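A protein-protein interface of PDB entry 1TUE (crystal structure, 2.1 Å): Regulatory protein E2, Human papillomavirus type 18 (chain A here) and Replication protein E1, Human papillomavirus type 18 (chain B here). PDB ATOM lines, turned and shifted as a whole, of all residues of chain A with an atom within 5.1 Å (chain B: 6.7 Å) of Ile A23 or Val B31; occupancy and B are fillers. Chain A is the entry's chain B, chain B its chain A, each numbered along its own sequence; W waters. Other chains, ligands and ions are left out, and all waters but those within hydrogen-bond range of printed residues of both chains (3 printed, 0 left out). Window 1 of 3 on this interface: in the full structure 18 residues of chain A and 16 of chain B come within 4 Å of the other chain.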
ATOM      1  N   GLN A  19      -1.400  18.054  23.480  1.00  0.00           N
ATOM      2  CA  GLN A  19      -2.391  18.810  24.245  1.00  0.00           C
ATOM      3  C   GLN A  19      -2.720  20.155  23.609  1.00  0.00           C
ATOM      4  O   GLN A  19      -3.866  20.577  23.652  1.00  0.00           O
ATOM      5  CB  GLN A  19      -1.974  18.948  25.706  1.00  0.00           C
ATOM      6  CG  GLN A  19      -1.977  17.596  26.422  1.00  0.00           C
ATOM      7  CD  GLN A  19      -1.744  17.696  27.905  1.00  0.00           C
ATOM      8  OE1 GLN A  19      -1.040  18.600  28.379  1.00  0.00           O
ATOM      9  NE2 GLN A  19      -2.331  16.764  28.655  1.00  0.00           N
ATOM     10  N   ASP A  20      -1.718  20.813  23.010  1.00  0.00           N
ATOM     11  CA  ASP A  20      -1.952  22.021  22.207  1.00  0.00           C
ATOM     12  C   ASP A  20      -2.910  21.734  21.044  1.00  0.00           C
ATOM     13  O   ASP A  20      -3.841  22.486  20.821  1.00  0.00           O
ATOM     14  CB  ASP A  20      -0.644  22.583  21.646  1.00  0.00           C
ATOM     15  CG  ASP A  20       0.166  23.352  22.677  1.00  0.00           C
ATOM     16  OD1 ASP A  20      -0.348  23.636  23.785  1.00  0.00           O
ATOM     17  OD2 ASP A  20       1.341  23.730  22.453  1.00  0.00           O
ATOM     18  N   LYS A  21      -2.653  20.646  20.315  1.00  0.00           N
ATOM     19  CA  LYS A  21      -3.503  20.193  19.201  1.00  0.00           C
ATOM     20  C   LYS A  21      -4.936  19.886  19.642  1.00  0.00           C
ATOM     21  O   LYS A  21      -5.889  20.202  18.937  1.00  0.00           O
ATOM     22  CB  LYS A  21      -2.926  18.911  18.618  1.00  0.00           C
ATOM     23  CG  LYS A  21      -2.609  18.936  17.156  1.00  0.00           C
ATOM     24  CD  LYS A  21      -1.096  18.734  16.983  1.00  0.00           C
ATOM     25  CE  LYS A  21      -0.790  17.590  16.003  1.00  0.00           C
ATOM     26  NZ  LYS A  21       0.326  16.714  16.490  1.00  0.00           N
ATOM     27  N   ILE A  22      -5.080  19.225  20.789  1.00  0.00           N
ATOM     28  CA  ILE A  22      -6.407  18.911  21.312  1.00  0.00           C
ATOM     29  C   ILE A  22      -7.233  20.198  21.490  1.00  0.00           C
ATOM     30  O   ILE A  22      -8.384  20.274  21.066  1.00  0.00           O
ATOM     31  CB  ILE A  22      -6.317  18.090  22.636  1.00  0.00           C
ATOM     32  CG1 ILE A  22      -5.899  16.640  22.332  1.00  0.00           C
ATOM     33  CG2 ILE A  22      -7.653  18.115  23.366  1.00  0.00           C
ATOM     34  CD1 ILE A  22      -5.228  15.914  23.490  1.00  0.00           C
ATOM     35  N   ILE A  23      -6.633  21.212  22.095  1.00  0.00           N
ATOM     36  CA  ILE A  23      -7.339  22.482  22.291  1.00  0.00           C
ATOM     37  C   ILE A  23      -7.573  23.233  20.959  1.00  0.00           C
ATOM     38  O   ILE A  23      -8.585  23.881  20.802  1.00  0.00           O
ATOM     39  CB  ILE A  23      -6.601  23.343  23.361  1.00  0.00           C
ATOM     40  CG1 ILE A  23      -6.619  22.598  24.706  1.00  0.00           C
ATOM     41  CG2 ILE A  23      -7.252  24.720  23.499  1.00  0.00           C
ATOM     42  CD1 ILE A  23      -5.830  23.263  25.775  1.00  0.00           C
ATOM     43  N   ASP A  24      -6.655  23.112  19.996  1.00  0.00           N
ATOM     44  CA  ASP A  24      -6.908  23.612  18.633  1.00  0.00           C
ATOM     45  C   ASP A  24      -8.234  23.079  18.094  1.00  0.00           C
ATOM     46  O   ASP A  24      -9.024  23.831  17.514  1.00  0.00           O
ATOM     47  CB  ASP A  24      -5.779  23.206  17.664  1.00  0.00           C
ATOM     48  CG  ASP A  24      -4.488  23.984  17.884  1.00  0.00           C
ATOM     49  OD1 ASP A  24      -4.515  25.048  18.521  1.00  0.00           O
ATOM     50  OD2 ASP A  24      -3.379  23.608  17.448  1.00  0.00           O
ATOM     51  N   HIS A  25      -8.473  21.777  18.267  1.00  0.00           N
ATOM     52  CA  HIS A  25      -9.732  21.159  17.843  1.00  0.00           C
ATOM     53  C   HIS A  25     -10.932  21.831  18.492  1.00  0.00           C
ATOM     54  O   HIS A  25     -11.934  22.108  17.829  1.00  0.00           O
ATOM     55  CB  HIS A  25      -9.740  19.667  18.180  1.00  0.00           C
ATOM     56  CG  HIS A  25      -9.111  18.818  17.124  1.00  0.00           C
ATOM     57  ND1 HIS A  25      -9.854  18.111  16.205  1.00  0.00           N
ATOM     58  CD2 HIS A  25      -7.813  18.573  16.830  1.00  0.00           C
ATOM     59  CE1 HIS A  25      -9.040  17.468  15.389  1.00  0.00           C
ATOM     60  NE2 HIS A  25      -7.799  17.727  15.747  1.00  0.00           N
ATOM     61  N   TYR A  26     -10.823  22.078  19.798  1.00  0.00           N
ATOM     62  CA  TYR A  26     -11.883  22.743  20.553  1.00  0.00           C
ATOM     63  C   TYR A  26     -12.134  24.150  20.022  1.00  0.00           C
ATOM     64  O   TYR A  26     -13.277  24.584  19.927  1.00  0.00           O
ATOM     65  CB  TYR A  26     -11.529  22.807  22.049  1.00  0.00           C
ATOM     66  CG  TYR A  26     -11.415  21.461  22.744  1.00  0.00           C
ATOM     67  CD1 TYR A  26     -12.149  20.354  22.310  1.00  0.00           C
ATOM     68  CD2 TYR A  26     -10.593  21.308  23.859  1.00  0.00           C
ATOM     69  CE1 TYR A  26     -12.050  19.125  22.956  1.00  0.00           C
ATOM     70  CE2 TYR A  26     -10.481  20.074  24.514  1.00  0.00           C
ATOM     71  CZ  TYR A  26     -11.202  18.999  24.053  1.00  0.00           C
ATOM     72  OH  TYR A  26     -11.096  17.800  24.693  1.00  0.00           O
ATOM     73  N   GLU A  27     -11.055  24.855  19.690  1.00  0.00           N
ATOM     74  CA  GLU A  27     -11.129  26.187  19.095  1.00  0.00           C
ATOM     75  C   GLU A  27     -11.773  26.179  17.709  1.00  0.00           C
ATOM     76  O   GLU A  27     -12.619  27.014  17.407  1.00  0.00           O
ATOM     77  CB  GLU A  27      -9.721  26.792  18.975  1.00  0.00           C
ATOM     78  CG  GLU A  27      -9.033  26.990  20.315  1.00  0.00           C
ATOM     79  CD  GLU A  27      -7.719  27.736  20.222  1.00  0.00           C
ATOM     80  OE1 GLU A  27      -7.234  28.186  21.289  1.00  0.00           O
ATOM     81  OE2 GLU A  27      -7.156  27.859  19.108  1.00  0.00           O
ATOM     82  N   ASN A  28     -11.332  25.250  16.868  1.00  0.00           N
ATOM     83  CA  ASN A  28     -11.795  25.171  15.469  1.00  0.00           C
ATOM     84  C   ASN A  28     -13.266  24.791  15.321  1.00  0.00           C
ATOM     85  O   ASN A  28     -13.957  25.342  14.471  1.00  0.00           O
ATOM     86  CB  ASN A  28     -10.956  24.170  14.688  1.00  0.00           C
ATOM     87  CG  ASN A  28      -9.507  24.581  14.545  1.00  0.00           C
ATOM     88  OD1 ASN A  28      -9.131  25.741  14.764  1.00  0.00           O
ATOM     89  ND2 ASN A  28      -8.679  23.622  14.159  1.00  0.00           N
ATOM     90  N   TRP B  27      -8.085  31.968  26.343  1.00  0.00           N
ATOM     91  CA  TRP B  27      -9.010  31.000  26.919  1.00  0.00           C
ATOM     92  C   TRP B  27      -8.289  29.718  27.349  1.00  0.00           C
ATOM     93  O   TRP B  27      -8.814  28.957  28.139  1.00  0.00           O
ATOM     94  CB  TRP B  27     -10.184  30.712  25.966  1.00  0.00           C
ATOM     95  CG  TRP B  27      -9.995  29.591  24.967  1.00  0.00           C
ATOM     96  CD1 TRP B  27      -8.930  29.391  24.126  1.00  0.00           C
ATOM     97  CD2 TRP B  27     -10.929  28.540  24.678  1.00  0.00           C
ATOM     98  NE1 TRP B  27      -9.137  28.271  23.355  1.00  0.00           N
ATOM     99  CE2 TRP B  27     -10.357  27.728  23.671  1.00  0.00           C
ATOM    100  CE3 TRP B  27     -12.197  28.198  25.174  1.00  0.00           C
ATOM    101  CZ2 TRP B  27     -11.008  26.596  23.150  1.00  0.00           C
ATOM    102  CZ3 TRP B  27     -12.843  27.069  24.654  1.00  0.00           C
ATOM    103  CH2 TRP B  27     -12.246  26.293  23.649  1.00  0.00           C
ATOM    104  N   ARG B  28      -7.081  29.503  26.830  1.00  0.00           N
ATOM    105  CA  ARG B  28      -6.376  28.220  26.998  1.00  0.00           C
ATOM    106  C   ARG B  28      -6.125  27.779  28.444  1.00  0.00           C
ATOM    107  O   ARG B  28      -6.360  26.622  28.751  1.00  0.00           O
ATOM    108  CB  ARG B  28      -5.092  28.140  26.157  1.00  0.00           C
ATOM    109  CG  ARG B  28      -5.354  28.098  24.644  1.00  0.00           C
ATOM    110  CD  ARG B  28      -4.187  27.546  23.791  1.00  0.00           C
ATOM    111  NE  ARG B  28      -4.690  27.270  22.447  1.00  0.00           N
ATOM    112  CZ  ARG B  28      -4.355  26.237  21.693  1.00  0.00           C
ATOM    113  NH1 ARG B  28      -3.477  25.333  22.105  1.00  0.00           N
ATOM    114  NH2 ARG B  28      -4.912  26.116  20.507  1.00  0.00           N
ATOM    115  N   PRO B  29      -5.674  28.672  29.333  1.00  0.00           N
ATOM    116  CA  PRO B  29      -5.474  28.286  30.736  1.00  0.00           C
ATOM    117  C   PRO B  29      -6.742  27.734  31.393  1.00  0.00           C
ATOM    118  O   PRO B  29      -6.654  26.863  32.249  1.00  0.00           O
ATOM    119  CB  PRO B  29      -5.034  29.591  31.419  1.00  0.00           C
ATOM    120  CG  PRO B  29      -4.512  30.471  30.300  1.00  0.00           C
ATOM    121  CD  PRO B  29      -5.300  30.083  29.086  1.00  0.00           C
ATOM    122  N   ILE B  30      -7.908  28.241  31.009  1.00  0.00           N
ATOM    123  CA  ILE B  30      -9.158  27.711  31.543  1.00  0.00           C
ATOM    124  C   ILE B  30      -9.366  26.263  31.081  1.00  0.00           C
ATOM    125  O   ILE B  30      -9.638  25.382  31.907  1.00  0.00           O
ATOM    126  CB  ILE B  30     -10.349  28.622  31.175  1.00  0.00           C
ATOM    127  CG1 ILE B  30     -10.215  29.975  31.917  1.00  0.00           C
ATOM    128  CG2 ILE B  30     -11.685  27.933  31.494  1.00  0.00           C
ATOM    129  CD1 ILE B  30     -11.197  31.030  31.451  1.00  0.00           C
ATOM    130  N   VAL B  31      -9.230  26.022  29.773  1.00  0.00           N
ATOM    131  CA  VAL B  31      -9.430  24.681  29.214  1.00  0.00           C
ATOM    132  C   VAL B  31      -8.389  23.742  29.802  1.00  0.00           C
ATOM    133  O   VAL B  31      -8.722  22.637  30.233  1.00  0.00           O
ATOM    134  CB  VAL B  31      -9.371  24.652  27.657  1.00  0.00           C
ATOM    135  CG1 VAL B  31      -9.651  23.228  27.123  1.00  0.00           C
ATOM    136  CG2 VAL B  31     -10.365  25.648  27.054  1.00  0.00           C
ATOM    137  N   GLN B  32      -7.141  24.210  29.858  1.00  0.00           N
ATOM    138  CA  GLN B  32      -6.044  23.395  30.330  1.00  0.00           C
ATOM    139  C   GLN B  32      -6.229  23.041  31.811  1.00  0.00           C
ATOM    140  O   GLN B  32      -5.905  21.928  32.223  1.00  0.00           O
ATOM    141  CB  GLN B  32      -4.692  24.099  30.095  1.00  0.00           C
ATOM    142  CG  GLN B  32      -4.319  24.276  28.600  1.00  0.00           C
ATOM    143  CD  GLN B  32      -3.226  25.323  28.352  1.00  0.00           C
ATOM    144  OE1 GLN B  32      -3.159  26.354  29.041  1.00  0.00           O
ATOM    145  NE2 GLN B  32      -2.366  25.057  27.368  1.00  0.00           N
ATOM    146  N   PHE B  33      -6.733  23.998  32.599  1.00  0.00           N
ATOM    147  CA  PHE B  33      -6.983  23.764  34.014  1.00  0.00           C
ATOM    148  C   PHE B  33      -8.072  22.710  34.228  1.00  0.00           C
ATOM    149  O   PHE B  33      -7.937  21.847  35.082  1.00  0.00           O
ATOM    150  CB  PHE B  33      -7.338  25.067  34.754  1.00  0.00           C
ATOM    151  CG  PHE B  33      -7.590  24.874  36.233  1.00  0.00           C
ATOM    152  CD1 PHE B  33      -6.581  24.389  37.066  1.00  0.00           C
ATOM    153  CD2 PHE B  33      -8.836  25.164  36.785  1.00  0.00           C
ATOM    154  CE1 PHE B  33      -6.809  24.209  38.439  1.00  0.00           C
ATOM    155  CE2 PHE B  33      -9.083  24.986  38.144  1.00  0.00           C
ATOM    156  CZ  PHE B  33      -8.059  24.509  38.986  1.00  0.00           C
ATOM    157  N   LEU B  34      -9.137  22.784  33.442  1.00  0.00           N
ATOM    158  CA  LEU B  34     -10.175  21.770  33.479  1.00  0.00           C
ATOM    159  C   LEU B  34      -9.621  20.373  33.175  1.00  0.00           C
ATOM    160  O   LEU B  34      -9.882  19.420  33.931  1.00  0.00           O
ATOM    161  CB  LEU B  34     -11.309  22.128  32.506  1.00  0.00           C
ATOM    162  CG  LEU B  34     -12.133  23.369  32.839  1.00  0.00           C
ATOM    163  CD1 LEU B  34     -12.997  23.740  31.645  1.00  0.00           C
ATOM    164  CD2 LEU B  34     -13.009  23.126  34.080  1.00  0.00           C
ATOM    165  N   ARG B  35      -8.845  20.259  32.090  1.00  0.00           N
ATOM    166  CA  ARG B  35      -8.269  18.953  31.702  1.00  0.00           C
ATOM    167  C   ARG B  35      -7.223  18.497  32.724  1.00  0.00           C
ATOM    168  O   ARG B  35      -7.106  17.307  33.003  1.00  0.00           O
ATOM    169  CB  ARG B  35      -7.673  18.994  30.289  1.00  0.00           C
ATOM    170  CG  ARG B  35      -8.667  19.480  29.200  1.00  0.00           C
ATOM    171  CD  ARG B  35      -8.200  19.199  27.752  1.00  0.00           C
ATOM    172  NE  ARG B  35      -8.307  17.774  27.438  1.00  0.00           N
ATOM    173  CZ  ARG B  35      -7.274  16.948  27.260  1.00  0.00           C
ATOM    174  NH1 ARG B  35      -6.021  17.393  27.335  1.00  0.00           N
ATOM    175  NH2 ARG B  35      -7.494  15.673  26.984  1.00  0.00           N
ATOM    176  N   TYR B  36      -6.483  19.448  33.288  1.00  0.00           N
ATOM    177  CA  TYR B  36      -5.598  19.153  34.418  1.00  0.00           C
ATOM    178  C   TYR B  36      -6.368  18.509  35.590  1.00  0.00           C
ATOM    179  O   TYR B  36      -5.860  17.589  36.244  1.00  0.00           O
ATOM    180  CB  TYR B  36      -4.852  20.407  34.886  1.00  0.00           C
ATOM    181  CG  TYR B  36      -4.126  20.213  36.211  1.00  0.00           C
ATOM    182  CD1 TYR B  36      -2.844  19.656  36.258  1.00  0.00           C
ATOM    183  CD2 TYR B  36      -4.730  20.584  37.417  1.00  0.00           C
ATOM    184  CE1 TYR B  36      -2.192  19.462  37.481  1.00  0.00           C
ATOM    185  CE2 TYR B  36      -4.090  20.398  38.631  1.00  0.00           C
ATOM    186  CZ  TYR B  36      -2.822  19.843  38.660  1.00  0.00           C
ATOM    187  OH  TYR B  36      -2.190  19.656  39.870  1.00  0.00           O
ATOM    188  N   ILE B  39     -11.281  16.884  33.916  1.00  0.00           N
ATOM    189  CA  ILE B  39     -12.637  17.218  33.494  1.00  0.00           C
ATOM    190  C   ILE B  39     -12.639  17.262  31.964  1.00  0.00           C
ATOM    191  O   ILE B  39     -11.703  17.792  31.351  1.00  0.00           O
ATOM    192  CB  ILE B  39     -13.087  18.557  34.148  1.00  0.00           C
ATOM    193  CG1 ILE B  39     -13.183  18.390  35.677  1.00  0.00           C
ATOM    194  CG2 ILE B  39     -14.406  19.044  33.562  1.00  0.00           C
ATOM    195  CD1 ILE B  39     -13.320  19.697  36.484  1.00  0.00           C
ATOM    196  N   PHE B  41     -13.672  18.717  28.592  1.00  0.00           N
ATOM    197  CA  PHE B  41     -14.109  20.008  28.050  1.00  0.00           C
ATOM    198  C   PHE B  41     -15.562  20.001  27.577  1.00  0.00           C
ATOM    199  O   PHE B  41     -16.346  20.832  28.017  1.00  0.00           O
ATOM    200  CB  PHE B  41     -13.181  20.508  26.915  1.00  0.00           C
ATOM    201  CG  PHE B  41     -13.703  21.738  26.199  1.00  0.00           C
ATOM    202  CD1 PHE B  41     -13.708  22.980  26.832  1.00  0.00           C
ATOM    203  CD2 PHE B  41     -14.223  21.643  24.917  1.00  0.00           C
ATOM    204  CE1 PHE B  41     -14.225  24.112  26.192  1.00  0.00           C
ATOM    205  CE2 PHE B  41     -14.746  22.776  24.255  1.00  0.00           C
ATOM    206  CZ  PHE B  41     -14.737  24.013  24.906  1.00  0.00           C
ATOM    207  N   PHE B  74     -11.031  29.340  41.003  1.00  0.00           N
ATOM    208  CA  PHE B  74     -11.587  29.131  39.665  1.00  0.00           C
ATOM    209  C   PHE B  74     -13.038  29.600  39.643  1.00  0.00           C
ATOM    210  O   PHE B  74     -13.432  30.382  38.778  1.00  0.00           O
ATOM    211  CB  PHE B  74     -11.482  27.646  39.297  1.00  0.00           C
ATOM    212  CG  PHE B  74     -12.066  27.295  37.951  1.00  0.00           C
ATOM    213  CD1 PHE B  74     -11.478  27.744  36.774  1.00  0.00           C
ATOM    214  CD2 PHE B  74     -13.184  26.478  37.861  1.00  0.00           C
ATOM    215  CE1 PHE B  74     -12.031  27.402  35.522  1.00  0.00           C
ATOM    216  CE2 PHE B  74     -13.730  26.126  36.614  1.00  0.00           C
ATOM    217  CZ  PHE B  74     -13.163  26.591  35.458  1.00  0.00           C
ATOM    218  N   PHE B 200     -12.780  32.973  26.566  1.00  0.00           N
ATOM    219  CA  PHE B 200     -13.502  31.704  26.681  1.00  0.00           C
ATOM    220  C   PHE B 200     -14.903  31.816  26.091  1.00  0.00           C
ATOM    221  O   PHE B 200     -15.321  30.966  25.313  1.00  0.00           O
ATOM    222  CB  PHE B 200     -13.546  31.229  28.151  1.00  0.00           C
ATOM    223  CG  PHE B 200     -14.256  29.905  28.352  1.00  0.00           C
ATOM    224  CD1 PHE B 200     -13.531  28.739  28.535  1.00  0.00           C
ATOM    225  CD2 PHE B 200     -15.648  29.840  28.375  1.00  0.00           C
ATOM    226  CE1 PHE B 200     -14.187  27.512  28.711  1.00  0.00           C
ATOM    227  CE2 PHE B 200     -16.309  28.614  28.547  1.00  0.00           C
ATOM    228  CZ  PHE B 200     -15.579  27.462  28.717  1.00  0.00           C
HETATM  229  O   HOH W   1     -11.336  17.462  27.266  1.00  0.00           O
HETATM  230  O   HOH W   2     -14.216  16.965  25.804  1.00  0.00           O
HETATM  231  O   HOH W   3      -2.552  22.432  26.279  1.00  0.00           O
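The indole nitrogen (NE1) of Trp B27 lies within hydrogen-bond range of the side-chain carboxylate (OE1) of Glu A27 (2.8 Å).
The guanidinium group (NH1) of Arg B28 lies within salt-bridge range of the side-chain carboxylate (OD1) of Asp A20, 3.9 Å away.
The guanidinium group (NH1) of Arg B28 is in salt-bridge range of the side-chain carboxylate (OD1) of Asp A24, at 3.7 Å.
NE of Arg B28 lies within salt-bridge range of OE1 of Glu A27 (2.9 Å).
O of Arg B28 lies close to OE1 of Gln B32 (3.2 Å).
O of Asp A24 lies close to OD1 of Asn A28 (3.3 Å).
Among the printed residues, pairs that only touch across the chains: Ile A23 with Gln B32 (3.4 Å), Tyr A26 with Phe B41 (3.6 Å), Ile A23 with Arg B28 (3.7 Å), Tyr A26 with Trp B27 (3.9 Å), Tyr A26 with Val B31 (3.9 Å), Tyr A26 with Arg B35 (3.9 Å), Ile A23 with Val B31 (3.9 Å) and Gln A19 with Arg B35 (3.97 Å).
Ile A23 touches just these residues of chain B: Arg B28 (3.7 Å), Val B31 (3.9 Å) and Gln B32 (3.4 Å).
Printed residues of chain B within 4 Å of Tyr A26: Trp B27, Val B31, Arg B35 and Phe B41.
Printed residues of chain A within 4 Å of Gln B32: Ile A23 (3.4 Å).
Of the printed residues of chain A, Trp B27 touches Tyr A26 and Glu A27.
Lys A21 touches none of the printed residues of chain B.
The nearest printed residue of chain A that does not touch Gln B32 is Asp A20 (4.4 Å).
Of the 14 printed residues of chain B, 6 touch a printed residue of chain A.
Along chain B the printed residues that touch a printed residue of chain A span positions 27 to 41.
Of the 10 printed residues of chain A, 6 touch a printed residue of chain B.
Hydrophobic or aromatic side chains of chain A within 4 Å of the printed part of chain B: Ile A23 and Tyr A26.
Among the printed residues, Asp or Glu carboxylates within 4 Å of a Lys or Arg side-chain nitrogen of the other chain: Asp A20 with Arg B28 (3.9 Å), Asp A24 with Arg B28 (2.3 Å) and Glu A27 with Arg B28 (2.9 Å).
Water W1 lies within hydrogen-bond range of the side-chain hydroxyl of Tyr A26 (2.6 Å), the backbone NH of Phe B41 (3.0 Å) and the guanidinium group of Arg B35 (3.0 Å).
Water W3 lies within hydrogen-bond range of the side-chain amide nitrogen (NE2) of Gln B32 (2.8 Å) and the backbone carbonyl oxygen (O) of Gln A19 (3.5 Å).
Water W2 bridges the backbone NH of Phe B41 (3.3 Å) and the side-chain hydroxyl of Tyr A26 (3.4 Å).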
